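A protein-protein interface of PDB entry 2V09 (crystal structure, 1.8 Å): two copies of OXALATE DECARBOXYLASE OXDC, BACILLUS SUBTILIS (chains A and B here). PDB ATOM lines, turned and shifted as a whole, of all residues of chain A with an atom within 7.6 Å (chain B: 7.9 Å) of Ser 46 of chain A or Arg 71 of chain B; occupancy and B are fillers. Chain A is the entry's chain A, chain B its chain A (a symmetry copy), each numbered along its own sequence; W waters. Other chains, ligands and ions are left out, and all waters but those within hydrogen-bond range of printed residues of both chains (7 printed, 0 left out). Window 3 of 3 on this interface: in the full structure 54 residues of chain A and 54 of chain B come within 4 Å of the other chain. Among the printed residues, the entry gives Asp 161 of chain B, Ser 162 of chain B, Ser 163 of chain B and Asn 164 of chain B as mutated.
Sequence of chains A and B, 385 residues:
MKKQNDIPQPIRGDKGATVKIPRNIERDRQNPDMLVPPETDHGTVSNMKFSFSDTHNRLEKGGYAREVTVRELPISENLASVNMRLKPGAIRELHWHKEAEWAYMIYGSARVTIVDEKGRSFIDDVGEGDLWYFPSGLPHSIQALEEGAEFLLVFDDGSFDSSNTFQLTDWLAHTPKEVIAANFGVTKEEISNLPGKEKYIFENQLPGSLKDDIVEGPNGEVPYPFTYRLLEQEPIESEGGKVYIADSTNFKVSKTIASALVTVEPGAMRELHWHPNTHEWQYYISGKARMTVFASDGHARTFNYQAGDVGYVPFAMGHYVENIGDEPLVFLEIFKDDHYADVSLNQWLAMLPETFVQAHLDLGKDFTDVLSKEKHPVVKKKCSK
Water W1 lies within hydrogen-bond range of O of Asn 47 of chain A (2.7 Å), O of Arg 71 of chain B (2.8 Å) and N of Ile 75 of chain A (3.1 Å). Water W4 lies within hydrogen-bond range of the backbone carbonyl oxygen (O) of Glu 72 of chain B (2.7 Å) and the backbone carbonyl oxygen (O) of Glu 72 of chain A (2.7 Å).
The side-chain hydroxyl (OG1) of Thr 44 of chain A sits at hydrogen-bond distance from the side-chain carboxylate (OD1) of Asp 161 of chain B. The backbone NH (N) of Asn 47 of chain A lies within hydrogen-bond range of the side-chain carboxylate (OE2) of Glu 72 of chain B, at 3.5 Å.
Glu 72 of chain B touches its own counterpart, Glu 72 of chain A. Pro 74 of chain B touches its own counterpart, Pro 74 of chain A. 4 positions are printed for both chains. Of the 10 pairs that touch across the chains among the printed residues, 2 have their exchanged pair printed and touching as well.
Among the printed residues, merely in contact across the chains: Asn 47 of chain A with Arg 71 of chain B, Pro 74 of chain A with Arg 71 of chain B, Ser 46 of chain A with Arg 71 of chain B, Thr 44 of chain A with Arg 71 of chain B, Asn 47 of chain A with Phe 50 of chain B, Pro 74 of chain A with Val 70 of chain B, Pro 74 of chain A with Pro 74 of chain B and Glu 72 of chain A with Glu 72 of chain B.
Of the 18 printed residues of chain A, 5 touch a printed residue of chain B. Hydrophobic or aromatic side chains of chain A within 4 Å of the printed part of chain B: Pro 74. Along chain A the printed residues that touch a printed residue of chain B span positions 44 to 74. Of the 20 printed residues of chain B, 6 touch a printed residue of chain A. Hydrophobic or aromatic side chains of chain B that line the printed part of chain A: Phe 50 and Pro 74. Among the printed residues, no Asp or Glu carboxylate lies within 4 Å of a Lys or Arg side-chain nitrogen of the other chain.
The side-chain carboxylate (OE2) of Glu 67 of chain B lies within salt-bridge range of the guanidinium group (NH2) of Arg 71 of chain B. NH2 of Arg 71 of chain B is in hydrogen-bond range of O of Phe 160 of chain B, 2.9 Å away.
Ser 46 of chain A touches just one residue of chain B: Arg 71. Arg 71 of chain B touches just these residues of chain A: Thr 44, Ser 46, Asn 47 and Pro 74. Printed residues of chain A within 4 Å of Glu 72 of chain B: Asn 47 (3.5 Å) and Glu 72 (3.9 Å). Printed residues of chain B within 4 Å of Pro 74 of chain A: Val 70, Arg 71 and Pro 74. Of the printed residues of chain B, Asn 47 of chain A touches Phe 50, Arg 71 and Glu 72. Pro 314 of chain A touches none of the printed residues of chain B. The nearest residue of chain B that does not touch Ser 46 of chain A is Glu 72 of chain B (4.3 Å). The nearest printed residue of chain B that does not touch Pro 74 of chain A is Glu 72 of chain B (4.5 Å).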
ATOM      1  N   GLY A  43      -6.293  32.110  -1.741  1.00  0.00           N
ATOM      2  CA  GLY A  43      -7.360  31.195  -1.522  1.00  0.00           C
ATOM      3  C   GLY A  43      -6.920  29.925  -0.828  1.00  0.00           C
ATOM      4  O   GLY A  43      -5.740  29.685  -0.641  1.00  0.00           O
ATOM      5  N   THR A  44      -7.883  29.108  -0.504  1.00  0.00           N
ATOM      6  CA  THR A  44      -7.617  27.836   0.172  1.00  0.00           C
ATOM      7  C   THR A  44      -7.442  26.770  -0.904  1.00  0.00           C
ATOM      8  O   THR A  44      -8.299  26.632  -1.777  1.00  0.00           O
ATOM      9  CB  THR A  44      -8.783  27.469   1.077  1.00  0.00           C
ATOM     10  OG1 THR A  44      -8.914  28.525   2.023  1.00  0.00           O
ATOM     11  CG2 THR A  44      -8.563  26.108   1.812  1.00  0.00           C
ATOM     12  N   VAL A  45      -6.322  26.056  -0.793  1.00  0.00           N
ATOM     13  CA  VAL A  45      -5.995  24.870  -1.609  1.00  0.00           C
ATOM     14  C   VAL A  45      -5.578  23.787  -0.586  1.00  0.00           C
ATOM     15  O   VAL A  45      -4.913  24.091   0.439  1.00  0.00           O
ATOM     16  CB  VAL A  45      -4.864  25.233  -2.601  1.00  0.00           C
ATOM     17  CG1 VAL A  45      -4.361  24.064  -3.411  1.00  0.00           C
ATOM     18  CG2 VAL A  45      -5.298  26.475  -3.499  1.00  0.00           C
ATOM     19  N   SER A  46      -6.007  22.552  -0.821  1.00  0.00           N
ATOM     20  CA  SER A  46      -5.579  21.437   0.032  1.00  0.00           C
ATOM     21  C   SER A  46      -4.061  21.225  -0.028  1.00  0.00           C
ATOM     22  O   SER A  46      -3.380  21.609  -0.994  1.00  0.00           O
ATOM     23  CB  SER A  46      -6.259  20.135  -0.363  1.00  0.00           C
ATOM     24  OG  SER A  46      -7.639  20.228  -0.107  1.00  0.00           O
ATOM     25  N   ASN A  47      -3.535  20.604   1.015  1.00  0.00           N
ATOM     26  CA  ASN A  47      -2.137  20.242   0.989  1.00  0.00           C
ATOM     27  C   ASN A  47      -1.810  19.268  -0.162  1.00  0.00           C
ATOM     28  O   ASN A  47      -2.469  18.248  -0.354  1.00  0.00           O
ATOM     29  CB  ASN A  47      -1.723  19.593   2.288  1.00  0.00           C
ATOM     30  CG  ASN A  47      -0.232  19.254   2.325  1.00  0.00           C
ATOM     31  OD1 ASN A  47       0.625  20.069   1.918  1.00  0.00           O
ATOM     32  ND2 ASN A  47       0.092  18.043   2.850  1.00  0.00           N
ATOM     33  N   MET A  48      -0.749  19.580  -0.887  1.00  0.00           N
ATOM     34  CA  MET A  48      -0.317  18.801  -2.036  1.00  0.00           C
ATOM     35  C   MET A  48       1.102  18.282  -1.905  1.00  0.00           C
ATOM     36  O   MET A  48       1.722  17.961  -2.934  1.00  0.00           O
ATOM     37  CB  MET A  48      -0.357  19.651  -3.318  1.00  0.00           C
ATOM     38  CG  MET A  48      -1.662  20.317  -3.644  1.00  0.00           C
ATOM     39  SD  MET A  48      -2.980  19.173  -3.887  1.00  0.00           S
ATOM     40  CE  MET A  48      -4.402  20.332  -4.076  1.00  0.00           C
ATOM     41  N   LYS A  49       1.590  18.144  -0.667  1.00  0.00           N
ATOM     42  CA  LYS A  49       3.015  17.799  -0.394  1.00  0.00           C
ATOM     43  C   LYS A  49       3.163  16.940   0.838  1.00  0.00           C
ATOM     44  O   LYS A  49       2.590  17.257   1.865  1.00  0.00           O
ATOM     45  CB  LYS A  49       3.795  19.119  -0.222  1.00  0.00           C
ATOM     46  CG  LYS A  49       5.182  19.045   0.361  1.00  0.00           C
ATOM     47  CD  LYS A  49       5.590  20.520   0.687  1.00  0.00           C
ATOM     48  CE  LYS A  49       6.768  20.586   1.665  1.00  0.00           C
ATOM     49  NZ  LYS A  49       8.043  20.372   0.967  1.00  0.00           N
ATOM     50  N   GLU A  72      -1.994  10.061   5.216  1.00  0.00           N
ATOM     51  CA  GLU A  72      -0.946  11.094   5.291  1.00  0.00           C
ATOM     52  C   GLU A  72      -1.257  12.324   4.387  1.00  0.00           C
ATOM     53  O   GLU A  72      -1.044  13.464   4.794  1.00  0.00           O
ATOM     54  CB  GLU A  72       0.407  10.511   4.802  1.00  0.00           C
ATOM     55  CG  GLU A  72       1.056   9.529   5.733  1.00  0.00           C
ATOM     56  CD  GLU A  72       0.287   8.222   5.959  1.00  0.00           C
ATOM     57  OE1 GLU A  72       0.060   7.452   4.977  1.00  0.00           O
ATOM     58  OE2 GLU A  72      -0.091   7.965   7.135  1.00  0.00           O
ATOM     59  N   LEU A  73      -1.741  12.058   3.171  1.00  0.00           N
ATOM     60  CA  LEU A  73      -1.971  13.045   2.095  1.00  0.00           C
ATOM     61  C   LEU A  73      -3.397  12.836   1.548  1.00  0.00           C
ATOM     62  O   LEU A  73      -3.598  12.072   0.573  1.00  0.00           O
ATOM     63  CB  LEU A  73      -0.946  12.823   0.970  1.00  0.00           C
ATOM     64  CG  LEU A  73      -0.958  13.856  -0.158  1.00  0.00           C
ATOM     65  CD1 LEU A  73      -0.601  15.288   0.380  1.00  0.00           C
ATOM     66  CD2 LEU A  73       0.002  13.409  -1.260  1.00  0.00           C
ATOM     67  N   PRO A  74      -4.389  13.432   2.214  1.00  0.00           N
ATOM     68  CA  PRO A  74      -5.808  13.078   1.975  1.00  0.00           C
ATOM     69  C   PRO A  74      -6.352  13.518   0.621  1.00  0.00           C
ATOM     70  O   PRO A  74      -7.328  12.939   0.162  1.00  0.00           O
ATOM     71  CB  PRO A  74      -6.563  13.780   3.115  1.00  0.00           C
ATOM     72  CG  PRO A  74      -5.646  14.920   3.537  1.00  0.00           C
ATOM     73  CD  PRO A  74      -4.245  14.459   3.286  1.00  0.00           C
ATOM     74  N   ILE A  75      -5.708  14.503  -0.027  1.00  0.00           N
ATOM     75  CA  ILE A  75      -6.052  14.867  -1.433  1.00  0.00           C
ATOM     76  C   ILE A  75      -5.901  13.652  -2.385  1.00  0.00           C
ATOM     77  O   ILE A  75      -6.612  13.503  -3.378  1.00  0.00           O
ATOM     78  CB  ILE A  75      -5.245  16.084  -1.925  1.00  0.00           C
ATOM     79  CG1 ILE A  75      -5.868  16.699  -3.200  1.00  0.00           C
ATOM     80  CG2 ILE A  75      -3.759  15.726  -2.109  1.00  0.00           C
ATOM     81  CD1 ILE A  75      -7.308  17.179  -3.015  1.00  0.00           C
ATOM     82  N   VAL A 293      -0.008  25.332  -8.140  1.00  0.00           N
ATOM     83  CA  VAL A 293      -1.227  24.622  -8.534  1.00  0.00           C
ATOM     84  C   VAL A 293      -2.366  25.675  -8.649  1.00  0.00           C
ATOM     85  O   VAL A 293      -2.669  26.390  -7.711  1.00  0.00           O
ATOM     86  CB  VAL A 293      -1.592  23.496  -7.536  1.00  0.00           C
ATOM     87  CG1 VAL A 293      -2.931  22.879  -7.847  1.00  0.00           C
ATOM     88  CG2 VAL A 293      -0.448  22.397  -7.471  1.00  0.00           C
ATOM     89  N   ALA A 295      -6.185  26.313  -9.175  1.00  0.00           N
ATOM     90  CA  ALA A 295      -7.342  25.552  -8.758  1.00  0.00           C
ATOM     91  C   ALA A 295      -8.670  26.125  -9.248  1.00  0.00           C
ATOM     92  O   ALA A 295      -9.699  25.594  -8.866  1.00  0.00           O
ATOM     93  CB  ALA A 295      -7.377  25.381  -7.211  1.00  0.00           C
ATOM     94  N   ARG A 301      -1.889  27.950  -5.245  1.00  0.00           N
ATOM     95  CA  ARG A 301      -1.005  27.785  -4.083  1.00  0.00           C
ATOM     96  C   ARG A 301       0.278  27.106  -4.563  1.00  0.00           C
ATOM     97  O   ARG A 301       0.242  26.166  -5.365  1.00  0.00           O
ATOM     98  CB  ARG A 301      -1.678  27.001  -2.930  1.00  0.00           C
ATOM     99  CG  ARG A 301      -0.807  26.817  -1.697  1.00  0.00           C
ATOM    100  CD  ARG A 301      -1.539  26.371  -0.440  1.00  0.00           C
ATOM    101  NE  ARG A 301      -2.568  27.304  -0.053  1.00  0.00           N
ATOM    102  CZ  ARG A 301      -3.226  27.237   1.098  1.00  0.00           C
ATOM    103  NH1 ARG A 301      -2.924  26.307   1.969  1.00  0.00           N
ATOM    104  NH2 ARG A 301      -4.171  28.121   1.353  1.00  0.00           N
ATOM    105  N   PHE A 303       3.912  25.178  -3.856  1.00  0.00           N
ATOM    106  CA  PHE A 303       4.524  24.166  -2.972  1.00  0.00           C
ATOM    107  C   PHE A 303       5.999  23.959  -3.381  1.00  0.00           C
ATOM    108  O   PHE A 303       6.378  24.099  -4.545  1.00  0.00           O
ATOM    109  CB  PHE A 303       3.778  22.819  -3.019  1.00  0.00           C
ATOM    110  CG  PHE A 303       2.345  22.899  -2.627  1.00  0.00           C
ATOM    111  CD1 PHE A 303       1.379  23.252  -3.565  1.00  0.00           C
ATOM    112  CD2 PHE A 303       1.957  22.702  -1.281  1.00  0.00           C
ATOM    113  CE1 PHE A 303       0.004  23.381  -3.189  1.00  0.00           C
ATOM    114  CE2 PHE A 303       0.614  22.844  -0.909  1.00  0.00           C
ATOM    115  CZ  PHE A 303      -0.354  23.149  -1.870  1.00  0.00           C
ATOM    116  N   TYR A 312       1.044  16.259  -5.591  1.00  0.00           N
ATOM    117  CA  TYR A 312      -0.240  15.945  -6.191  1.00  0.00           C
ATOM    118  C   TYR A 312      -0.793  17.192  -6.926  1.00  0.00           C
ATOM    119  O   TYR A 312      -0.582  18.348  -6.477  1.00  0.00           O
ATOM    120  CB  TYR A 312      -1.237  15.468  -5.114  1.00  0.00           C
ATOM    121  CG  TYR A 312      -2.380  14.576  -5.599  1.00  0.00           C
ATOM    122  CD1 TYR A 312      -2.203  13.204  -5.777  1.00  0.00           C
ATOM    123  CD2 TYR A 312      -3.659  15.091  -5.839  1.00  0.00           C
ATOM    124  CE1 TYR A 312      -3.244  12.386  -6.169  1.00  0.00           C
ATOM    125  CE2 TYR A 312      -4.693  14.265  -6.262  1.00  0.00           C
ATOM    126  CZ  TYR A 312      -4.481  12.922  -6.445  1.00  0.00           C
ATOM    127  OH  TYR A 312      -5.516  12.068  -6.831  1.00  0.00           O
ATOM    128  N   PRO A 314      -4.594  17.871  -8.439  1.00  0.00           N
ATOM    129  CA  PRO A 314      -5.960  17.398  -8.780  1.00  0.00           C
ATOM    130  C   PRO A 314      -6.300  17.661 -10.258  1.00  0.00           C
ATOM    131  O   PRO A 314      -5.791  18.623 -10.866  1.00  0.00           O
ATOM    132  CB  PRO A 314      -6.846  18.202  -7.812  1.00  0.00           C
ATOM    133  CG  PRO A 314      -5.956  18.544  -6.685  1.00  0.00           C
ATOM    134  CD  PRO A 314      -4.624  18.830  -7.342  1.00  0.00           C
ATOM    135  N   MET A 317      -6.178  20.797 -12.930  1.00  0.00           N
ATOM    136  CA  MET A 317      -5.592  22.017 -12.359  1.00  0.00           C
ATOM    137  C   MET A 317      -4.319  22.431 -13.133  1.00  0.00           C
ATOM    138  O   MET A 317      -3.516  21.604 -13.549  1.00  0.00           O
ATOM    139  CB  MET A 317      -5.304  21.856 -10.853  1.00  0.00           C
ATOM    140  CG  MET A 317      -6.596  21.772 -10.019  1.00  0.00           C
ATOM    141  SD  MET A 317      -6.324  21.991  -8.286  1.00  0.00           S
ATOM    142  CE  MET A 317      -8.051  21.897  -7.690  1.00  0.00           C
ATOM    143  N   PHE B  50       1.988  17.015  12.009  1.00  0.00           N
ATOM    144  CA  PHE B  50       2.084  17.939  10.862  1.00  0.00           C
ATOM    145  C   PHE B  50       2.753  19.248  11.354  1.00  0.00           C
ATOM    146  O   PHE B  50       2.381  19.735  12.466  1.00  0.00           O
ATOM    147  CB  PHE B  50       0.719  18.208  10.205  1.00  0.00           C
ATOM    148  CG  PHE B  50       0.826  18.598   8.754  1.00  0.00           C
ATOM    149  CD1 PHE B  50       1.008  19.938   8.431  1.00  0.00           C
ATOM    150  CD2 PHE B  50       0.862  17.636   7.724  1.00  0.00           C
ATOM    151  CE1 PHE B  50       1.184  20.345   7.143  1.00  0.00           C
ATOM    152  CE2 PHE B  50       1.039  18.067   6.353  1.00  0.00           C
ATOM    153  CZ  PHE B  50       1.198  19.407   6.088  1.00  0.00           C
ATOM    154  N   GLU B  67      -2.330  27.792   8.502  1.00  0.00           N
ATOM    155  CA  GLU B  67      -3.329  26.874   9.099  1.00  0.00           C
ATOM    156  C   GLU B  67      -2.996  25.395   8.913  1.00  0.00           C
ATOM    157  O   GLU B  67      -2.391  24.985   7.893  1.00  0.00           O
ATOM    158  CB  GLU B  67      -4.727  27.158   8.558  1.00  0.00           C
ATOM    159  CG  GLU B  67      -4.887  26.949   7.062  1.00  0.00           C
ATOM    160  CD  GLU B  67      -6.327  27.209   6.527  1.00  0.00           C
ATOM    161  OE1 GLU B  67      -7.112  27.952   7.184  1.00  0.00           O
ATOM    162  OE2 GLU B  67      -6.686  26.656   5.460  1.00  0.00           O
ATOM    163  N   VAL B  68      -3.368  24.613   9.929  1.00  0.00           N
ATOM    164  CA  VAL B  68      -3.333  23.171   9.845  1.00  0.00           C
ATOM    165  C   VAL B  68      -4.773  22.702  10.096  1.00  0.00           C
ATOM    166  O   VAL B  68      -5.326  22.886  11.186  1.00  0.00           O
ATOM    167  CB  VAL B  68      -2.316  22.517  10.808  1.00  0.00           C
ATOM    168  CG1 VAL B  68      -2.438  20.986  10.727  1.00  0.00           C
ATOM    169  CG2 VAL B  68      -0.857  23.006  10.464  1.00  0.00           C
ATOM    170  N   THR B  69      -5.336  22.118   9.058  1.00  0.00           N
ATOM    171  CA  THR B  69      -6.722  21.636   9.017  1.00  0.00           C
ATOM    172  C   THR B  69      -6.771  20.137   8.610  1.00  0.00           C
ATOM    173  O   THR B  69      -5.737  19.503   8.404  1.00  0.00           O
ATOM    174  CB  THR B  69      -7.581  22.495   7.992  1.00  0.00           C
ATOM    175  OG1 THR B  69      -7.334  22.053   6.620  1.00  0.00           O
ATOM    176  CG2 THR B  69      -7.325  24.015   8.188  1.00  0.00           C
ATOM    177  N   VAL B  70      -7.980  19.607   8.474  1.00  0.00           N
ATOM    178  CA  VAL B  70      -8.220  18.230   8.026  1.00  0.00           C
ATOM    179  C   VAL B  70      -7.678  18.021   6.590  1.00  0.00           C
ATOM    180  O   VAL B  70      -7.431  16.883   6.184  1.00  0.00           O
ATOM    181  CB  VAL B  70      -9.751  17.877   8.119  1.00  0.00           C
ATOM    182  CG1 VAL B  70     -10.542  18.570   6.984  1.00  0.00           C
ATOM    183  CG2 VAL B  70     -10.017  16.362   8.197  1.00  0.00           C
ATOM    184  N   ARG B  71      -7.490  19.107   5.825  1.00  0.00           N
ATOM    185  CA  ARG B  71      -6.882  19.023   4.494  1.00  0.00           C
ATOM    186  C   ARG B  71      -5.358  18.776   4.553  1.00  0.00           C
ATOM    187  O   ARG B  71      -4.740  18.403   3.560  1.00  0.00           O
ATOM    188  CB  ARG B  71      -7.203  20.293   3.704  1.00  0.00           C
ATOM    189  CG  ARG B  71      -8.723  20.516   3.548  1.00  0.00           C
ATOM    190  CD  ARG B  71      -9.045  21.798   2.823  1.00  0.00           C
ATOM    191  NE  ARG B  71      -8.665  22.965   3.606  1.00  0.00           N
ATOM    192  CZ  ARG B  71      -9.381  23.476   4.617  1.00  0.00           C
ATOM    193  NH1 ARG B  71     -10.544  22.931   4.966  1.00  0.00           N
ATOM    194  NH2 ARG B  71      -8.935  24.568   5.226  1.00  0.00           N
ATOM    195  N   GLU B  72      -4.768  18.985   5.738  1.00  0.00           N
ATOM    196  CA  GLU B  72      -3.349  18.698   6.015  1.00  0.00           C
ATOM    197  C   GLU B  72      -3.161  17.431   6.901  1.00  0.00           C
ATOM    198  O   GLU B  72      -2.265  16.626   6.653  1.00  0.00           O
ATOM    199  CB  GLU B  72      -2.712  19.883   6.788  1.00  0.00           C
ATOM    200  CG  GLU B  72      -2.489  21.129   5.981  1.00  0.00           C
ATOM    201  CD  GLU B  72      -3.755  21.820   5.465  1.00  0.00           C
ATOM    202  OE1 GLU B  72      -4.608  22.264   6.293  1.00  0.00           O
ATOM    203  OE2 GLU B  72      -3.895  21.921   4.215  1.00  0.00           O
ATOM    204  N   LEU B  73      -4.005  17.295   7.928  1.00  0.00           N
ATOM    205  CA  LEU B  73      -3.927  16.262   8.982  1.00  0.00           C
ATOM    206  C   LEU B  73      -5.321  15.618   9.126  1.00  0.00           C
ATOM    207  O   LEU B  73      -6.147  16.071   9.955  1.00  0.00           O
ATOM    208  CB  LEU B  73      -3.518  16.917  10.311  1.00  0.00           C
ATOM    209  CG  LEU B  73      -3.256  15.961  11.476  1.00  0.00           C
ATOM    210  CD1 LEU B  73      -2.054  15.000  11.160  1.00  0.00           C
ATOM    211  CD2 LEU B  73      -3.015  16.771  12.749  1.00  0.00           C
ATOM    212  N   PRO B  74      -5.617  14.632   8.276  1.00  0.00           N
ATOM    213  CA  PRO B  74      -7.005  14.137   8.114  1.00  0.00           C
ATOM    214  C   PRO B  74      -7.548  13.368   9.314  1.00  0.00           C
ATOM    215  O   PRO B  74      -8.761  13.286   9.460  1.00  0.00           O
ATOM    216  CB  PRO B  74      -6.933  13.229   6.876  1.00  0.00           C
ATOM    217  CG  PRO B  74      -5.472  12.808   6.794  1.00  0.00           C
ATOM    218  CD  PRO B  74      -4.669  13.936   7.360  1.00  0.00           C
ATOM    219  N   ILE B  75      -6.664  12.846  10.180  1.00  0.00           N
ATOM    220  CA  ILE B  75      -7.102  12.245  11.474  1.00  0.00           C
ATOM    221  C   ILE B  75      -7.887  13.268  12.335  1.00  0.00           C
ATOM    222  O   ILE B  75      -8.791  12.929  13.097  1.00  0.00           O
ATOM    223  CB  ILE B  75      -5.922  11.629  12.250  1.00  0.00           C
ATOM    224  CG1 ILE B  75      -6.412  10.678  13.366  1.00  0.00           C
ATOM    225  CG2 ILE B  75      -4.977  12.723  12.781  1.00  0.00           C
ATOM    226  CD1 ILE B  75      -7.254   9.508  12.855  1.00  0.00           C
ATOM    227  N   SER B  76      -7.566  14.551  12.167  1.00  0.00           N
ATOM    228  CA  SER B  76      -8.171  15.595  12.995  1.00  0.00           C
ATOM    229  C   SER B  76      -9.390  16.230  12.329  1.00  0.00           C
ATOM    230  O   SER B  76      -9.328  17.333  11.776  1.00  0.00           O
ATOM    231  CB  SER B  76      -7.131  16.667  13.369  1.00  0.00           C
ATOM    232  OG  SER B  76      -7.704  17.621  14.247  1.00  0.00           O
ATOM    233  N   ALA B  80      -9.237  22.268  14.177  1.00  0.00           N
ATOM    234  CA  ALA B  80      -8.319  22.852  13.223  1.00  0.00           C
ATOM    235  C   ALA B  80      -7.628  24.050  13.905  1.00  0.00           C
ATOM    236  O   ALA B  80      -8.072  24.495  14.973  1.00  0.00           O
ATOM    237  CB  ALA B  80      -9.038  23.282  11.911  1.00  0.00           C
ATOM    238  N   ASP B 157     -13.973  22.768  14.406  1.00  0.00           N
ATOM    239  CA  ASP B 157     -14.271  21.915  13.269  1.00  0.00           C
ATOM    240  C   ASP B 157     -12.971  21.743  12.456  1.00  0.00           C
ATOM    241  O   ASP B 157     -12.344  22.715  12.096  1.00  0.00           O
ATOM    242  CB  ASP B 157     -15.412  22.539  12.458  1.00  0.00           C
ATOM    243  CG  ASP B 157     -15.894  21.680  11.272  1.00  0.00           C
ATOM    244  OD1 ASP B 157     -15.330  20.605  10.961  1.00  0.00           O
ATOM    245  OD2 ASP B 157     -16.897  22.100  10.654  1.00  0.00           O
ATOM    246  N   GLY B 158     -12.612  20.505  12.163  1.00  0.00           N
ATOM    247  CA  GLY B 158     -11.378  20.206  11.388  1.00  0.00           C
ATOM    248  C   GLY B 158     -11.480  20.725   9.953  1.00  0.00           C
ATOM    249  O   GLY B 158     -10.477  20.972   9.292  1.00  0.00           O
ATOM    250  N   SER B 159     -12.719  20.907   9.482  1.00  0.00           N
ATOM    251  CA  SER B 159     -12.967  21.406   8.145  1.00  0.00           C
ATOM    252  C   SER B 159     -12.897  22.927   8.037  1.00  0.00           C
ATOM    253  O   SER B 159     -13.088  23.475   6.941  1.00  0.00           O
ATOM    254  CB  SER B 159     -14.317  20.909   7.630  1.00  0.00           C
ATOM    255  OG  SER B 159     -14.202  19.531   7.423  1.00  0.00           O
ATOM    256  N   PHE B 160     -12.625  23.613   9.147  1.00  0.00           N
ATOM    257  CA  PHE B 160     -12.425  25.061   9.148  1.00  0.00           C
ATOM    258  C   PHE B 160     -11.638  25.540   7.929  1.00  0.00           C
ATOM    259  O   PHE B 160     -10.582  24.988   7.580  1.00  0.00           O
ATOM    260  CB  PHE B 160     -11.694  25.504  10.439  1.00  0.00           C
ATOM    261  CG  PHE B 160     -11.330  26.959  10.461  1.00  0.00           C
ATOM    262  CD1 PHE B 160     -12.208  27.912  10.974  1.00  0.00           C
ATOM    263  CD2 PHE B 160     -10.079  27.364  10.042  1.00  0.00           C
ATOM    264  CE1 PHE B 160     -11.833  29.268  11.030  1.00  0.00           C
ATOM    265  CE2 PHE B 160      -9.728  28.707  10.073  1.00  0.00           C
ATOM    266  CZ  PHE B 160     -10.603  29.633  10.585  1.00  0.00           C
ATOM    267  N   ASP B 161     -12.138  26.613   7.323  1.00  0.00           N
ATOM    268  CA  ASP B 161     -11.513  27.213   6.150  1.00  0.00           C
ATOM    269  C   ASP B 161     -11.442  28.719   6.409  1.00  0.00           C
ATOM    270  O   ASP B 161     -12.482  29.369   6.489  1.00  0.00           O
ATOM    271  CB  ASP B 161     -12.345  26.901   4.918  1.00  0.00           C
ATOM    272  CG  ASP B 161     -11.700  27.403   3.599  1.00  0.00           C
ATOM    273  OD1 ASP B 161     -10.910  28.349   3.608  1.00  0.00           O
ATOM    274  OD2 ASP B 161     -12.015  26.786   2.571  1.00  0.00           O
ATOM    275  N   SER B 162     -10.217  29.197   6.577  1.00  0.00           N
ATOM    276  CA  SER B 162      -9.867  30.576   6.919  1.00  0.00           C
ATOM    277  C   SER B 162     -10.601  31.590   6.042  1.00  0.00           C
ATOM    278  O   SER B 162     -10.477  32.810   6.329  1.00  0.00           O
ATOM    279  CB  SER B 162      -8.350  30.818   6.797  1.00  0.00           C
ATOM    280  OG  SER B 162      -7.545  30.274   7.861  1.00  0.00           O
ATOM    281  N   SER B 163     -11.350  31.135   5.013  1.00  0.00           N
ATOM    282  CA  SER B 163     -12.303  32.001   4.354  1.00  0.00           C
ATOM    283  C   SER B 163     -13.794  31.685   4.164  1.00  0.00           C
ATOM    284  O   SER B 163     -14.506  32.467   3.510  1.00  0.00           O
ATOM    285  CB  SER B 163     -11.784  32.448   3.050  1.00  0.00           C
ATOM    286  OG  SER B 163     -12.439  33.669   2.808  1.00  0.00           O
ATOM    287  N   ASN B 164     -14.293  30.614   4.722  1.00  0.00           N
ATOM    288  CA  ASN B 164     -15.665  30.619   5.086  1.00  0.00           C
ATOM    289  C   ASN B 164     -15.865  31.760   6.178  1.00  0.00           C
ATOM    290  O   ASN B 164     -16.985  31.906   6.652  1.00  0.00           O
ATOM    291  CB  ASN B 164     -16.135  29.279   5.740  1.00  0.00           C
ATOM    292  CG  ASN B 164     -16.170  28.055   4.800  1.00  0.00           C
ATOM    293  OD1 ASN B 164     -16.044  28.152   3.562  1.00  0.00           O
ATOM    294  ND2 ASN B 164     -16.361  26.851   5.439  1.00  0.00           N
HETATM  295  O   HOH W   1      -4.248  16.924   1.215  1.00  0.00           O
HETATM  296  O   HOH W   2      -5.961  28.851   3.381  1.00  0.00           O
HETATM  297  O   HOH W   3      -5.824  23.541   3.082  1.00  0.00           O
HETATM  298  O   HOH W   4      -1.150  14.254   7.424  1.00  0.00           O
HETATM  299  O   HOH W   5      -2.482  25.208   5.205  1.00  0.00           O
HETATM  300  O   HOH W   6      -4.815  25.748   4.099  1.00  0.00           O
HETATM  301  O   HOH W   7      -1.245  16.112   4.153  1.00  0.00           O
